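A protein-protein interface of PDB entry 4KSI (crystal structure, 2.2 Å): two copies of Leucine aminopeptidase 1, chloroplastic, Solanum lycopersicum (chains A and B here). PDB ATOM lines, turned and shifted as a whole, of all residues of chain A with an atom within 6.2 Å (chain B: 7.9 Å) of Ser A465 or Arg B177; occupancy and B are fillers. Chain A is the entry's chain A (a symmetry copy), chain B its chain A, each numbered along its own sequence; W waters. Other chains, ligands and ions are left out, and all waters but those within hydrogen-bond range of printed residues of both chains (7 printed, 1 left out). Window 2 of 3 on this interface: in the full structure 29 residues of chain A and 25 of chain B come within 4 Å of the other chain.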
ATOM      1  N   ILE A 370     -14.005  19.638 -13.225  1.00  0.00           N
ATOM      2  CA  ILE A 370     -13.454  19.041 -14.437  1.00  0.00           C
ATOM      3  C   ILE A 370     -12.392  18.043 -14.065  1.00  0.00           C
ATOM      4  O   ILE A 370     -11.426  18.420 -13.387  1.00  0.00           O
ATOM      5  CB  ILE A 370     -12.899  20.108 -15.405  1.00  0.00           C
ATOM      6  CG1 ILE A 370     -14.048  21.038 -15.871  1.00  0.00           C
ATOM      7  CG2 ILE A 370     -12.157  19.414 -16.579  1.00  0.00           C
ATOM      8  CD1 ILE A 370     -13.602  22.234 -16.714  1.00  0.00           C
ATOM      9  N   THR A 378     -10.588  15.645 -20.933  1.00  0.00           N
ATOM     10  CA  THR A 378     -11.164  16.289 -19.792  1.00  0.00           C
ATOM     11  C   THR A 378     -12.679  16.088 -19.825  1.00  0.00           C
ATOM     12  O   THR A 378     -13.306  16.079 -20.910  1.00  0.00           O
ATOM     13  CB  THR A 378     -10.841  17.783 -19.802  1.00  0.00           C
ATOM     14  OG1 THR A 378     -11.277  18.337 -21.049  1.00  0.00           O
ATOM     15  CG2 THR A 378      -9.310  18.020 -19.702  1.00  0.00           C
ATOM     16  N   GLU A 380     -16.273  17.385 -17.899  1.00  0.00           N
ATOM     17  CA  GLU A 380     -16.991  18.254 -16.974  1.00  0.00           C
ATOM     18  C   GLU A 380     -18.054  17.343 -16.329  1.00  0.00           C
ATOM     19  O   GLU A 380     -18.919  16.804 -17.037  1.00  0.00           O
ATOM     20  CB  GLU A 380     -17.685  19.403 -17.720  1.00  0.00           C
ATOM     21  CG  GLU A 380     -18.434  20.337 -16.761  1.00  0.00           C
ATOM     22  CD  GLU A 380     -19.136  21.512 -17.477  1.00  0.00           C
ATOM     23  OE1 GLU A 380     -19.307  21.524 -18.767  1.00  0.00           O
ATOM     24  OE2 GLU A 380     -19.545  22.469 -16.733  1.00  0.00           O
ATOM     25  N   MET A 463     -23.677  15.864 -25.650  1.00  0.00           N
ATOM     26  CA  MET A 463     -22.612  15.612 -24.611  1.00  0.00           C
ATOM     27  C   MET A 463     -21.499  16.653 -24.632  1.00  0.00           C
ATOM     28  O   MET A 463     -20.443  16.490 -23.976  1.00  0.00           O
ATOM     29  CB  MET A 463     -21.985  14.205 -24.719  1.00  0.00           C
ATOM     30  CG  MET A 463     -23.032  13.089 -24.622  1.00  0.00           C
ATOM     31  SD  MET A 463     -23.784  13.093 -22.960  1.00  0.00           S
ATOM     32  CE  MET A 463     -22.559  12.184 -21.973  1.00  0.00           C
ATOM     33  N   LYS A 464     -21.696  17.701 -25.397  1.00  0.00           N
ATOM     34  CA  LYS A 464     -20.718  18.782 -25.517  1.00  0.00           C
ATOM     35  C   LYS A 464     -20.668  19.616 -24.228  1.00  0.00           C
ATOM     36  O   LYS A 464     -21.723  19.832 -23.600  1.00  0.00           O
ATOM     37  CB  LYS A 464     -21.077  19.686 -26.706  1.00  0.00           C
ATOM     38  CG  LYS A 464     -20.924  19.014 -28.068  1.00  0.00           C
ATOM     39  CD  LYS A 464     -20.388  19.972 -29.131  1.00  0.00           C
ATOM     40  CE  LYS A 464     -21.456  20.465 -30.082  1.00  0.00           C
ATOM     41  NZ  LYS A 464     -20.899  21.352 -31.160  1.00  0.00           N
ATOM     42  N   SER A 465     -19.482  20.117 -23.876  1.00  0.00           N
ATOM     43  CA  SER A 465     -19.286  20.965 -22.713  1.00  0.00           C
ATOM     44  C   SER A 465     -18.934  22.363 -23.199  1.00  0.00           C
ATOM     45  O   SER A 465     -18.295  22.515 -24.266  1.00  0.00           O
ATOM     46  CB  SER A 465     -18.109  20.399 -21.879  1.00  0.00           C
ATOM     47  OG  SER A 465     -17.734  21.307 -20.864  1.00  0.00           O
ATOM     48  N   GLY A 466     -19.266  23.398 -22.410  1.00  0.00           N
ATOM     49  CA  GLY A 466     -18.799  24.747 -22.786  1.00  0.00           C
ATOM     50  C   GLY A 466     -17.352  25.028 -22.335  1.00  0.00           C
ATOM     51  O   GLY A 466     -16.806  26.138 -22.576  1.00  0.00           O
ATOM     52  N   VAL A 467     -16.717  24.034 -21.692  1.00  0.00           N
ATOM     53  CA  VAL A 467     -15.434  24.280 -21.024  1.00  0.00           C
ATOM     54  C   VAL A 467     -14.465  23.090 -21.104  1.00  0.00           C
ATOM     55  O   VAL A 467     -13.249  23.268 -21.286  1.00  0.00           O
ATOM     56  CB  VAL A 467     -15.651  24.786 -19.539  1.00  0.00           C
ATOM     57  CG1 VAL A 467     -16.354  23.742 -18.670  1.00  0.00           C
ATOM     58  CG2 VAL A 467     -14.346  25.148 -18.895  1.00  0.00           C
ATOM     59  N   ALA A 468     -14.977  21.868 -21.019  1.00  0.00           N
ATOM     60  CA  ALA A 468     -14.099  20.644 -21.113  1.00  0.00           C
ATOM     61  C   ALA A 468     -14.250  19.948 -22.464  1.00  0.00           C
ATOM     62  O   ALA A 468     -15.012  20.404 -23.299  1.00  0.00           O
ATOM     63  CB  ALA A 468     -14.460  19.654 -20.009  1.00  0.00           C
ATOM     64  N   ASP A 469     -13.567  18.813 -22.659  1.00  0.00           N
ATOM     65  CA  ASP A 469     -13.782  18.072 -23.898  1.00  0.00           C
ATOM     66  C   ASP A 469     -15.242  17.496 -23.985  1.00  0.00           C
ATOM     67  O   ASP A 469     -15.759  17.333 -25.106  1.00  0.00           O
ATOM     68  CB  ASP A 469     -12.821  16.922 -24.004  1.00  0.00           C
ATOM     69  CG  ASP A 469     -11.351  17.396 -24.130  1.00  0.00           C
ATOM     70  OD1 ASP A 469     -11.076  18.501 -24.629  1.00  0.00           O
ATOM     71  OD2 ASP A 469     -10.467  16.591 -23.810  1.00  0.00           O
ATOM     72  N   MET A 470     -15.887  17.187 -22.840  1.00  0.00           N
ATOM     73  CA  MET A 470     -17.238  16.630 -22.891  1.00  0.00           C
ATOM     74  C   MET A 470     -17.826  16.766 -21.485  1.00  0.00           C
ATOM     75  O   MET A 470     -17.058  17.035 -20.503  1.00  0.00           O
ATOM     76  CB  MET A 470     -17.165  15.122 -23.282  1.00  0.00           C
ATOM     77  CG  MET A 470     -16.448  14.281 -22.221  1.00  0.00           C
ATOM     78  SD  MET A 470     -15.889  12.658 -22.782  1.00  0.00           S
ATOM     79  CE  MET A 470     -14.495  13.134 -23.814  1.00  0.00           C
ATOM     80  N   ILE A 471     -19.138  16.537 -21.361  1.00  0.00           N
ATOM     81  CA  ILE A 471     -19.781  16.412 -20.076  1.00  0.00           C
ATOM     82  C   ILE A 471     -19.936  14.918 -19.800  1.00  0.00           C
ATOM     83  O   ILE A 471     -19.766  14.100 -20.707  1.00  0.00           O
ATOM     84  CB  ILE A 471     -21.162  17.142 -20.002  1.00  0.00           C
ATOM     85  CG1 ILE A 471     -22.173  16.546 -21.013  1.00  0.00           C
ATOM     86  CG2 ILE A 471     -20.982  18.680 -20.141  1.00  0.00           C
ATOM     87  CD1 ILE A 471     -23.542  17.298 -21.124  1.00  0.00           C
ATOM     88  N   THR B  20      -6.507  17.520 -12.965  1.00  0.00           N
ATOM     89  CA  THR B  20      -6.673  18.478 -14.036  1.00  0.00           C
ATOM     90  C   THR B  20      -5.654  19.616 -13.961  1.00  0.00           C
ATOM     91  O   THR B  20      -5.452  20.200 -12.896  1.00  0.00           O
ATOM     92  CB  THR B  20      -8.126  19.013 -14.026  1.00  0.00           C
ATOM     93  OG1 THR B  20      -8.994  17.904 -14.272  1.00  0.00           O
ATOM     94  CG2 THR B  20      -8.360  20.154 -15.081  1.00  0.00           C
ATOM     95  N   ARG B  21      -5.043  19.892 -15.117  1.00  0.00           N
ATOM     96  CA  ARG B  21      -4.066  20.981 -15.268  1.00  0.00           C
ATOM     97  C   ARG B  21      -4.569  21.980 -16.310  1.00  0.00           C
ATOM     98  O   ARG B  21      -4.725  21.647 -17.428  1.00  0.00           O
ATOM     99  CB  ARG B  21      -2.708  20.429 -15.703  1.00  0.00           C
ATOM    100  CG  ARG B  21      -1.543  21.412 -15.650  1.00  0.00           C
ATOM    101  N   PRO B  22      -4.819  23.208 -15.924  1.00  0.00           N
ATOM    102  CA  PRO B  22      -5.161  24.161 -17.005  1.00  0.00           C
ATOM    103  C   PRO B  22      -4.055  24.402 -18.074  1.00  0.00           C
ATOM    104  O   PRO B  22      -2.871  24.439 -17.751  1.00  0.00           O
ATOM    105  CB  PRO B  22      -5.404  25.489 -16.271  1.00  0.00           C
ATOM    106  CG  PRO B  22      -5.045  25.237 -14.847  1.00  0.00           C
ATOM    107  CD  PRO B  22      -4.460  23.858 -14.661  1.00  0.00           C
ATOM    108  N   ASN B  23      -4.453  24.551 -19.331  1.00  0.00           N
ATOM    109  CA  ASN B  23      -3.521  25.036 -20.344  1.00  0.00           C
ATOM    110  C   ASN B  23      -3.204  26.536 -20.089  1.00  0.00           C
ATOM    111  O   ASN B  23      -3.816  27.188 -19.233  1.00  0.00           O
ATOM    112  CB  ASN B  23      -4.085  24.790 -21.762  1.00  0.00           C
ATOM    113  CG  ASN B  23      -4.534  23.327 -22.005  1.00  0.00           C
ATOM    114  OD1 ASN B  23      -5.659  23.054 -22.482  1.00  0.00           O
ATOM    115  ND2 ASN B  23      -3.692  22.413 -21.690  1.00  0.00           N
ATOM    116  N   ASP B  26      -5.944  32.091 -22.476  1.00  0.00           N
ATOM    117  CA  ASP B  26      -6.337  32.619 -23.800  1.00  0.00           C
ATOM    118  C   ASP B  26      -6.754  34.090 -23.817  1.00  0.00           C
ATOM    119  O   ASP B  26      -7.447  34.483 -24.772  1.00  0.00           O
ATOM    120  CB  ASP B  26      -7.464  31.779 -24.447  1.00  0.00           C
ATOM    121  CG  ASP B  26      -7.055  30.313 -24.622  1.00  0.00           C
ATOM    122  OD1 ASP B  26      -6.304  30.043 -25.604  1.00  0.00           O
ATOM    123  OD2 ASP B  26      -7.458  29.460 -23.756  1.00  0.00           O
ATOM    124  N   PHE B 171     -12.533  36.553 -27.119  1.00  0.00           N
ATOM    125  CA  PHE B 171     -12.033  35.683 -26.050  1.00  0.00           C
ATOM    126  C   PHE B 171     -12.698  34.311 -26.097  1.00  0.00           C
ATOM    127  O   PHE B 171     -13.931  34.215 -26.047  1.00  0.00           O
ATOM    128  CB  PHE B 171     -12.302  36.317 -24.704  1.00  0.00           C
ATOM    129  CG  PHE B 171     -11.864  35.483 -23.519  1.00  0.00           C
ATOM    130  CD1 PHE B 171     -10.520  35.159 -23.325  1.00  0.00           C
ATOM    131  CD2 PHE B 171     -12.795  35.039 -22.591  1.00  0.00           C
ATOM    132  CE1 PHE B 171     -10.124  34.379 -22.235  1.00  0.00           C
ATOM    133  CE2 PHE B 171     -12.404  34.278 -21.496  1.00  0.00           C
ATOM    134  CZ  PHE B 171     -11.079  33.966 -21.314  1.00  0.00           C
ATOM    135  N   GLU B 172     -11.898  33.247 -26.200  1.00  0.00           N
ATOM    136  CA  GLU B 172     -12.440  31.902 -26.057  1.00  0.00           C
ATOM    137  C   GLU B 172     -11.592  31.183 -24.998  1.00  0.00           C
ATOM    138  O   GLU B 172     -10.411  31.061 -25.150  1.00  0.00           O
ATOM    139  CB  GLU B 172     -12.414  31.135 -27.390  1.00  0.00           C
ATOM    140  CG  GLU B 172     -13.443  29.994 -27.457  1.00  0.00           C
ATOM    141  CD  GLU B 172     -13.380  29.118 -28.759  1.00  0.00           C
ATOM    142  OE1 GLU B 172     -12.282  28.848 -29.352  1.00  0.00           O
ATOM    143  OE2 GLU B 172     -14.468  28.653 -29.179  1.00  0.00           O
ATOM    144  N   ASP B 173     -12.199  30.712 -23.927  1.00  0.00           N
ATOM    145  CA  ASP B 173     -11.455  30.136 -22.826  1.00  0.00           C
ATOM    146  C   ASP B 173     -11.227  28.628 -23.103  1.00  0.00           C
ATOM    147  O   ASP B 173     -12.142  27.829 -22.943  1.00  0.00           O
ATOM    148  CB  ASP B 173     -12.244  30.338 -21.552  1.00  0.00           C
ATOM    149  CG  ASP B 173     -11.440  29.975 -20.299  1.00  0.00           C
ATOM    150  OD1 ASP B 173     -10.312  29.428 -20.390  1.00  0.00           O
ATOM    151  OD2 ASP B 173     -11.935  30.235 -19.188  1.00  0.00           O
ATOM    152  N   ASN B 174     -10.011  28.240 -23.470  1.00  0.00           N
ATOM    153  CA  ASN B 174      -9.722  26.864 -23.804  1.00  0.00           C
ATOM    154  C   ASN B 174      -8.770  26.208 -22.819  1.00  0.00           C
ATOM    155  O   ASN B 174      -8.164  25.186 -23.149  1.00  0.00           O
ATOM    156  CB  ASN B 174      -9.178  26.741 -25.237  1.00  0.00           C
ATOM    157  CG  ASN B 174     -10.227  27.111 -26.288  1.00  0.00           C
ATOM    158  OD1 ASN B 174      -9.928  27.840 -27.201  1.00  0.00           O
ATOM    159  ND2 ASN B 174     -11.441  26.661 -26.133  1.00  0.00           N
ATOM    160  N   ARG B 175      -8.675  26.752 -21.609  1.00  0.00           N
ATOM    161  CA  ARG B 175      -7.756  26.198 -20.615  1.00  0.00           C
ATOM    162  C   ARG B 175      -8.045  24.741 -20.240  1.00  0.00           C
ATOM    163  O   ARG B 175      -7.141  24.023 -19.795  1.00  0.00           O
ATOM    164  CB  ARG B 175      -7.794  27.071 -19.384  1.00  0.00           C
ATOM    165  CG  ARG B 175      -7.132  28.441 -19.649  1.00  0.00           C
ATOM    166  CD  ARG B 175      -7.261  29.282 -18.356  1.00  0.00           C
ATOM    167  NE  ARG B 175      -8.702  29.505 -18.095  1.00  0.00           N
ATOM    168  CZ  ARG B 175      -9.205  29.799 -16.906  1.00  0.00           C
ATOM    169  NH1 ARG B 175      -8.364  29.956 -15.862  1.00  0.00           N
ATOM    170  NH2 ARG B 175     -10.527  29.948 -16.758  1.00  0.00           N
ATOM    171  N   PHE B 176      -9.299  24.296 -20.361  1.00  0.00           N
ATOM    172  CA  PHE B 176      -9.642  22.921 -19.899  1.00  0.00           C
ATOM    173  C   PHE B 176     -10.037  21.954 -20.996  1.00  0.00           C
ATOM    174  O   PHE B 176     -10.621  20.896 -20.749  1.00  0.00           O
ATOM    175  CB  PHE B 176     -10.679  23.018 -18.794  1.00  0.00           C
ATOM    176  CG  PHE B 176     -10.267  23.968 -17.709  1.00  0.00           C
ATOM    177  CD1 PHE B 176      -9.380  23.559 -16.704  1.00  0.00           C
ATOM    178  CD2 PHE B 176     -10.737  25.269 -17.693  1.00  0.00           C
ATOM    179  CE1 PHE B 176      -8.981  24.444 -15.719  1.00  0.00           C
ATOM    180  CE2 PHE B 176     -10.301  26.181 -16.726  1.00  0.00           C
ATOM    181  CZ  PHE B 176      -9.418  25.771 -15.732  1.00  0.00           C
ATOM    182  N   ARG B 177      -9.722  22.340 -22.226  1.00  0.00           N
ATOM    183  CA  ARG B 177     -10.020  21.546 -23.400  1.00  0.00           C
ATOM    184  C   ARG B 177      -8.718  20.992 -23.924  1.00  0.00           C
ATOM    185  O   ARG B 177      -7.727  21.731 -24.016  1.00  0.00           O
ATOM    186  CB  ARG B 177     -10.635  22.405 -24.501  1.00  0.00           C
ATOM    187  CG  ARG B 177     -12.068  22.780 -24.254  1.00  0.00           C
ATOM    188  CD  ARG B 177     -12.713  23.350 -25.501  1.00  0.00           C
ATOM    189  NE  ARG B 177     -12.856  24.797 -25.427  1.00  0.00           N
ATOM    190  CZ  ARG B 177     -14.010  25.439 -25.280  1.00  0.00           C
ATOM    191  NH1 ARG B 177     -14.000  26.752 -25.267  1.00  0.00           N
ATOM    192  NH2 ARG B 177     -15.163  24.777 -25.168  1.00  0.00           N
ATOM    193  N   SER B 178      -8.721  19.710 -24.273  1.00  0.00           N
ATOM    194  CA  SER B 178      -7.471  19.007 -24.568  1.00  0.00           C
ATOM    195  C   SER B 178      -7.007  19.298 -25.985  1.00  0.00           C
ATOM    196  O   SER B 178      -5.843  19.075 -26.305  1.00  0.00           O
ATOM    197  CB  SER B 178      -7.539  17.481 -24.268  1.00  0.00           C
ATOM    198  OG  SER B 178      -8.294  16.763 -25.232  1.00  0.00           O
ATOM    199  N   GLU B 179      -7.899  19.801 -26.812  1.00  0.00           N
ATOM    200  CA  GLU B 179      -7.558  20.143 -28.151  1.00  0.00           C
ATOM    201  C   GLU B 179      -8.465  21.287 -28.406  1.00  0.00           C
ATOM    202  O   GLU B 179      -9.647  21.214 -28.051  1.00  0.00           O
ATOM    203  CB  GLU B 179      -7.924  18.997 -29.086  1.00  0.00           C
ATOM    204  N   SER B 180      -7.923  22.331 -29.037  1.00  0.00           N
ATOM    205  CA  SER B 180      -8.641  23.559 -29.407  1.00  0.00           C
ATOM    206  C   SER B 180      -7.722  24.454 -30.304  1.00  0.00           C
ATOM    207  O   SER B 180      -6.498  24.209 -30.383  1.00  0.00           O
ATOM    208  CB  SER B 180      -8.985  24.327 -28.141  1.00  0.00           C
ATOM    209  OG  SER B 180      -7.774  24.782 -27.532  1.00  0.00           O
ATOM    210  N   LYS B 181      -8.281  25.475 -30.962  1.00  0.00           N
ATOM    211  CA  LYS B 181      -7.464  26.344 -31.830  1.00  0.00           C
ATOM    212  C   LYS B 181      -7.276  27.695 -31.168  1.00  0.00           C
ATOM    213  O   LYS B 181      -8.250  28.293 -30.741  1.00  0.00           O
ATOM    214  CB  LYS B 181      -8.108  26.541 -33.219  1.00  0.00           C
ATOM    215  CG  LYS B 181      -8.016  25.346 -34.169  1.00  0.00           C
ATOM    216  N   ASN B 221     -15.305  30.833 -14.944  1.00  0.00           N
ATOM    217  CA  ASN B 221     -15.266  29.653 -15.865  1.00  0.00           C
ATOM    218  C   ASN B 221     -14.605  28.459 -15.186  1.00  0.00           C
ATOM    219  O   ASN B 221     -15.077  27.314 -15.265  1.00  0.00           O
ATOM    220  CB  ASN B 221     -14.463  29.955 -17.173  1.00  0.00           C
ATOM    221  CG  ASN B 221     -15.277  30.693 -18.227  1.00  0.00           C
ATOM    222  OD1 ASN B 221     -16.517  30.617 -18.245  1.00  0.00           O
ATOM    223  ND2 ASN B 221     -14.569  31.418 -19.139  1.00  0.00           N
ATOM    224  N   LYS B 323     -19.974  26.686  -9.322  1.00  0.00           N
ATOM    225  CA  LYS B 323     -18.665  27.361  -9.387  1.00  0.00           C
ATOM    226  C   LYS B 323     -18.890  28.874  -9.632  1.00  0.00           C
ATOM    227  O   LYS B 323     -17.959  29.668  -9.418  1.00  0.00           O
ATOM    228  CB  LYS B 323     -17.812  26.806 -10.550  1.00  0.00           C
ATOM    229  CG  LYS B 323     -18.407  27.106 -11.946  1.00  0.00           C
ATOM    230  CD  LYS B 323     -17.560  26.482 -13.087  1.00  0.00           C
ATOM    231  CE  LYS B 323     -18.173  26.839 -14.461  1.00  0.00           C
ATOM    232  NZ  LYS B 323     -17.429  26.082 -15.555  1.00  0.00           N
ATOM    233  N   LYS B 511     -24.275  30.914 -24.071  1.00  0.00           N
ATOM    234  CA  LYS B 511     -22.881  30.672 -24.401  1.00  0.00           C
ATOM    235  C   LYS B 511     -22.241  29.554 -23.572  1.00  0.00           C
ATOM    236  O   LYS B 511     -21.093  29.207 -23.825  1.00  0.00           O
ATOM    237  CB  LYS B 511     -22.059  31.959 -24.247  1.00  0.00           C
ATOM    238  CG  LYS B 511     -22.310  32.986 -25.347  1.00  0.00           C
ATOM    239  CD  LYS B 511     -21.765  34.356 -24.954  1.00  0.00           C
ATOM    240  CE  LYS B 511     -22.057  35.421 -26.008  1.00  0.00           C
ATOM    241  NZ  LYS B 511     -21.549  36.748 -25.533  1.00  0.00           N
ATOM    242  N   LYS B 512     -22.941  29.058 -22.537  1.00  0.00           N
ATOM    243  CA  LYS B 512     -22.338  28.159 -21.513  1.00  0.00           C
ATOM    244  C   LYS B 512     -20.984  28.708 -20.992  1.00  0.00           C
ATOM    245  O   LYS B 512     -19.967  28.009 -21.031  1.00  0.00           O
ATOM    246  CB  LYS B 512     -22.165  26.708 -22.064  1.00  0.00           C
ATOM    247  CG  LYS B 512     -23.497  26.044 -22.400  1.00  0.00           C
ATOM    248  CD  LYS B 512     -23.376  24.606 -22.868  1.00  0.00           C
ATOM    249  CE  LYS B 512     -24.781  24.021 -22.951  1.00  0.00           C
ATOM    250  NZ  LYS B 512     -24.708  22.725 -23.639  1.00  0.00           N
ATOM    251  N   ASN B 513     -20.950  29.969 -20.567  1.00  0.00           N
ATOM    252  CA  ASN B 513     -19.684  30.608 -20.164  1.00  0.00           C
ATOM    253  C   ASN B 513     -19.995  31.802 -19.212  1.00  0.00           C
ATOM    254  O   ASN B 513     -21.154  32.299 -19.193  1.00  0.00           O
ATOM    255  CB  ASN B 513     -18.930  31.065 -21.439  1.00  0.00           C
ATOM    256  CG  ASN B 513     -17.431  30.684 -21.461  1.00  0.00           C
ATOM    257  OD1 ASN B 513     -16.582  31.565 -21.445  1.00  0.00           O
ATOM    258  ND2 ASN B 513     -17.110  29.403 -21.594  1.00  0.00           N
HETATM  259  O   HOH W   1     -24.417  19.789 -24.268  1.00  0.00           O
HETATM  260  O   HOH W   2     -12.190  19.837 -26.742  1.00  0.00           O
HETATM  261  O   HOH W   3     -22.922  21.379 -21.514  1.00  0.00           O
HETATM  262  O   HOH W   4     -14.774  27.858 -22.011  1.00  0.00           O
HETATM  263  O   HOH W   5     -11.607  25.422 -21.481  1.00  0.00           O
HETATM  264  O   HOH W   6     -19.873  24.991 -17.323  1.00  0.00           O
HETATM  265  O   HOH W   7     -17.725  23.337 -14.949  1.00  0.00           O
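Of the printed residues of chain B, Ser A465 touches Arg B177.
Of the printed residues of chain B, Ile A370 touches Thr B20 (2.6 Å) and Phe B176 (3.7 Å).
Printed residues of chain A within 4 Å of Lys B512: Gly A466.
The nearest printed residue of chain B that does not touch Ser A465 is Lys B512 (5.0 Å).
No position is printed for both chains.
The side-chain amide oxygen (OD1) of Asn B23 sits close to the backbone carbonyl oxygen (O) of Arg B177.
The side-chain amide nitrogen (ND2) of Asn B221 lies within hydrogen-bond range of the side-chain amide oxygen (OD1) of Asn B513 (3.1 Å).
N of Asp A469 is in hydrogen-bond range of OG1 of Thr A378 (2.8 Å).
The side-chain hydroxyl of Ser A465 is in hydrogen-bond range of the side-chain carboxylate of Glu A380 (2.6 Å).
The backbone NH (N) of Val A467 sits at hydrogen-bond distance from the side-chain hydroxyl (OG) of Ser A465 (3.0 Å).
N of Ala A468 sits at hydrogen-bond distance from OG of Ser A465, 2.8 Å away.
Among the printed residues, merely in contact across the chains: Ile A370 with Phe B176 (3.7 Å), Ser A465 with Arg B177 (3.97 Å), Gly A466 with Lys B512 (3.9 Å), Val A467 with Phe B176 (3.5 Å), Val A467 with Arg B177 (3.2 Å), Ala A468 with Phe B176 (3.5 Å), Ala A468 with Arg B177 (3.9 Å) and Asp A469 with Arg B177 (3.4 Å).
Water W6 bridges the side-chain carboxylate of Glu A380 (2.6 Å) and the side-chain amino group of Lys B323 (3.2 Å).
Water W7 lies within hydrogen-bond range of the side-chain carboxylate of Glu A380 (2.7 Å) and the side-chain amino group of Lys B323 (2.8 Å).
Water W5 lies within hydrogen-bond range of the backbone carbonyl oxygen of Val A467, the backbone NH of Phe B176, the backbone carbonyl oxygen of Asp B173 and the backbone NH of Arg B175.
Water W4 lies within hydrogen-bond range of O of Gly A466 (2.7 Å), O of Asp B173 (2.8 Å) and ND2 of Asn B513 (2.8 Å).
Water W2 bridges OD1 of Asp A469 (2.7 Å) and O of Glu B179 (3.2 Å).
Water W3 bridges O of Lys A464 and NZ of Lys B512.
Of the 21 printed residues of chain B, 6 touch a printed residue of chain A.
Hydrophobic or aromatic side chains of chain B that line the printed part of chain A: Phe B176.
Of the 12 printed residues of chain A, 7 touch a printed residue of chain B.
Printed residues of chain A that touch a printed residue of chain B: Ile A370, Thr A378, Ser A465, Gly A466, Val A467, Ala A468 and Asp A469.
Among the printed residues, 13 pairs touch across the chains.
Among the printed residues, no Asp or Glu carboxylate lies within 4 Å of a Lys or Arg side-chain nitrogen of the other chain.
OG1 of Thr B20 sits at hydrogen-bond distance from O of Ile A370, at 2.6 Å.
OG1 of Thr A378 is in hydrogen-bond range of O of Phe B176, 2.7 Å away.
NH2 of Arg B177 lies within hydrogen-bond range of O of Gly A466 (3.4 Å).
OD2 of Asp A469 sits at hydrogen-bond distance from OG of Ser B178, 2.6 Å away.
ND2 of Asn B513 lies within hydrogen-bond range of O of Gly A466.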
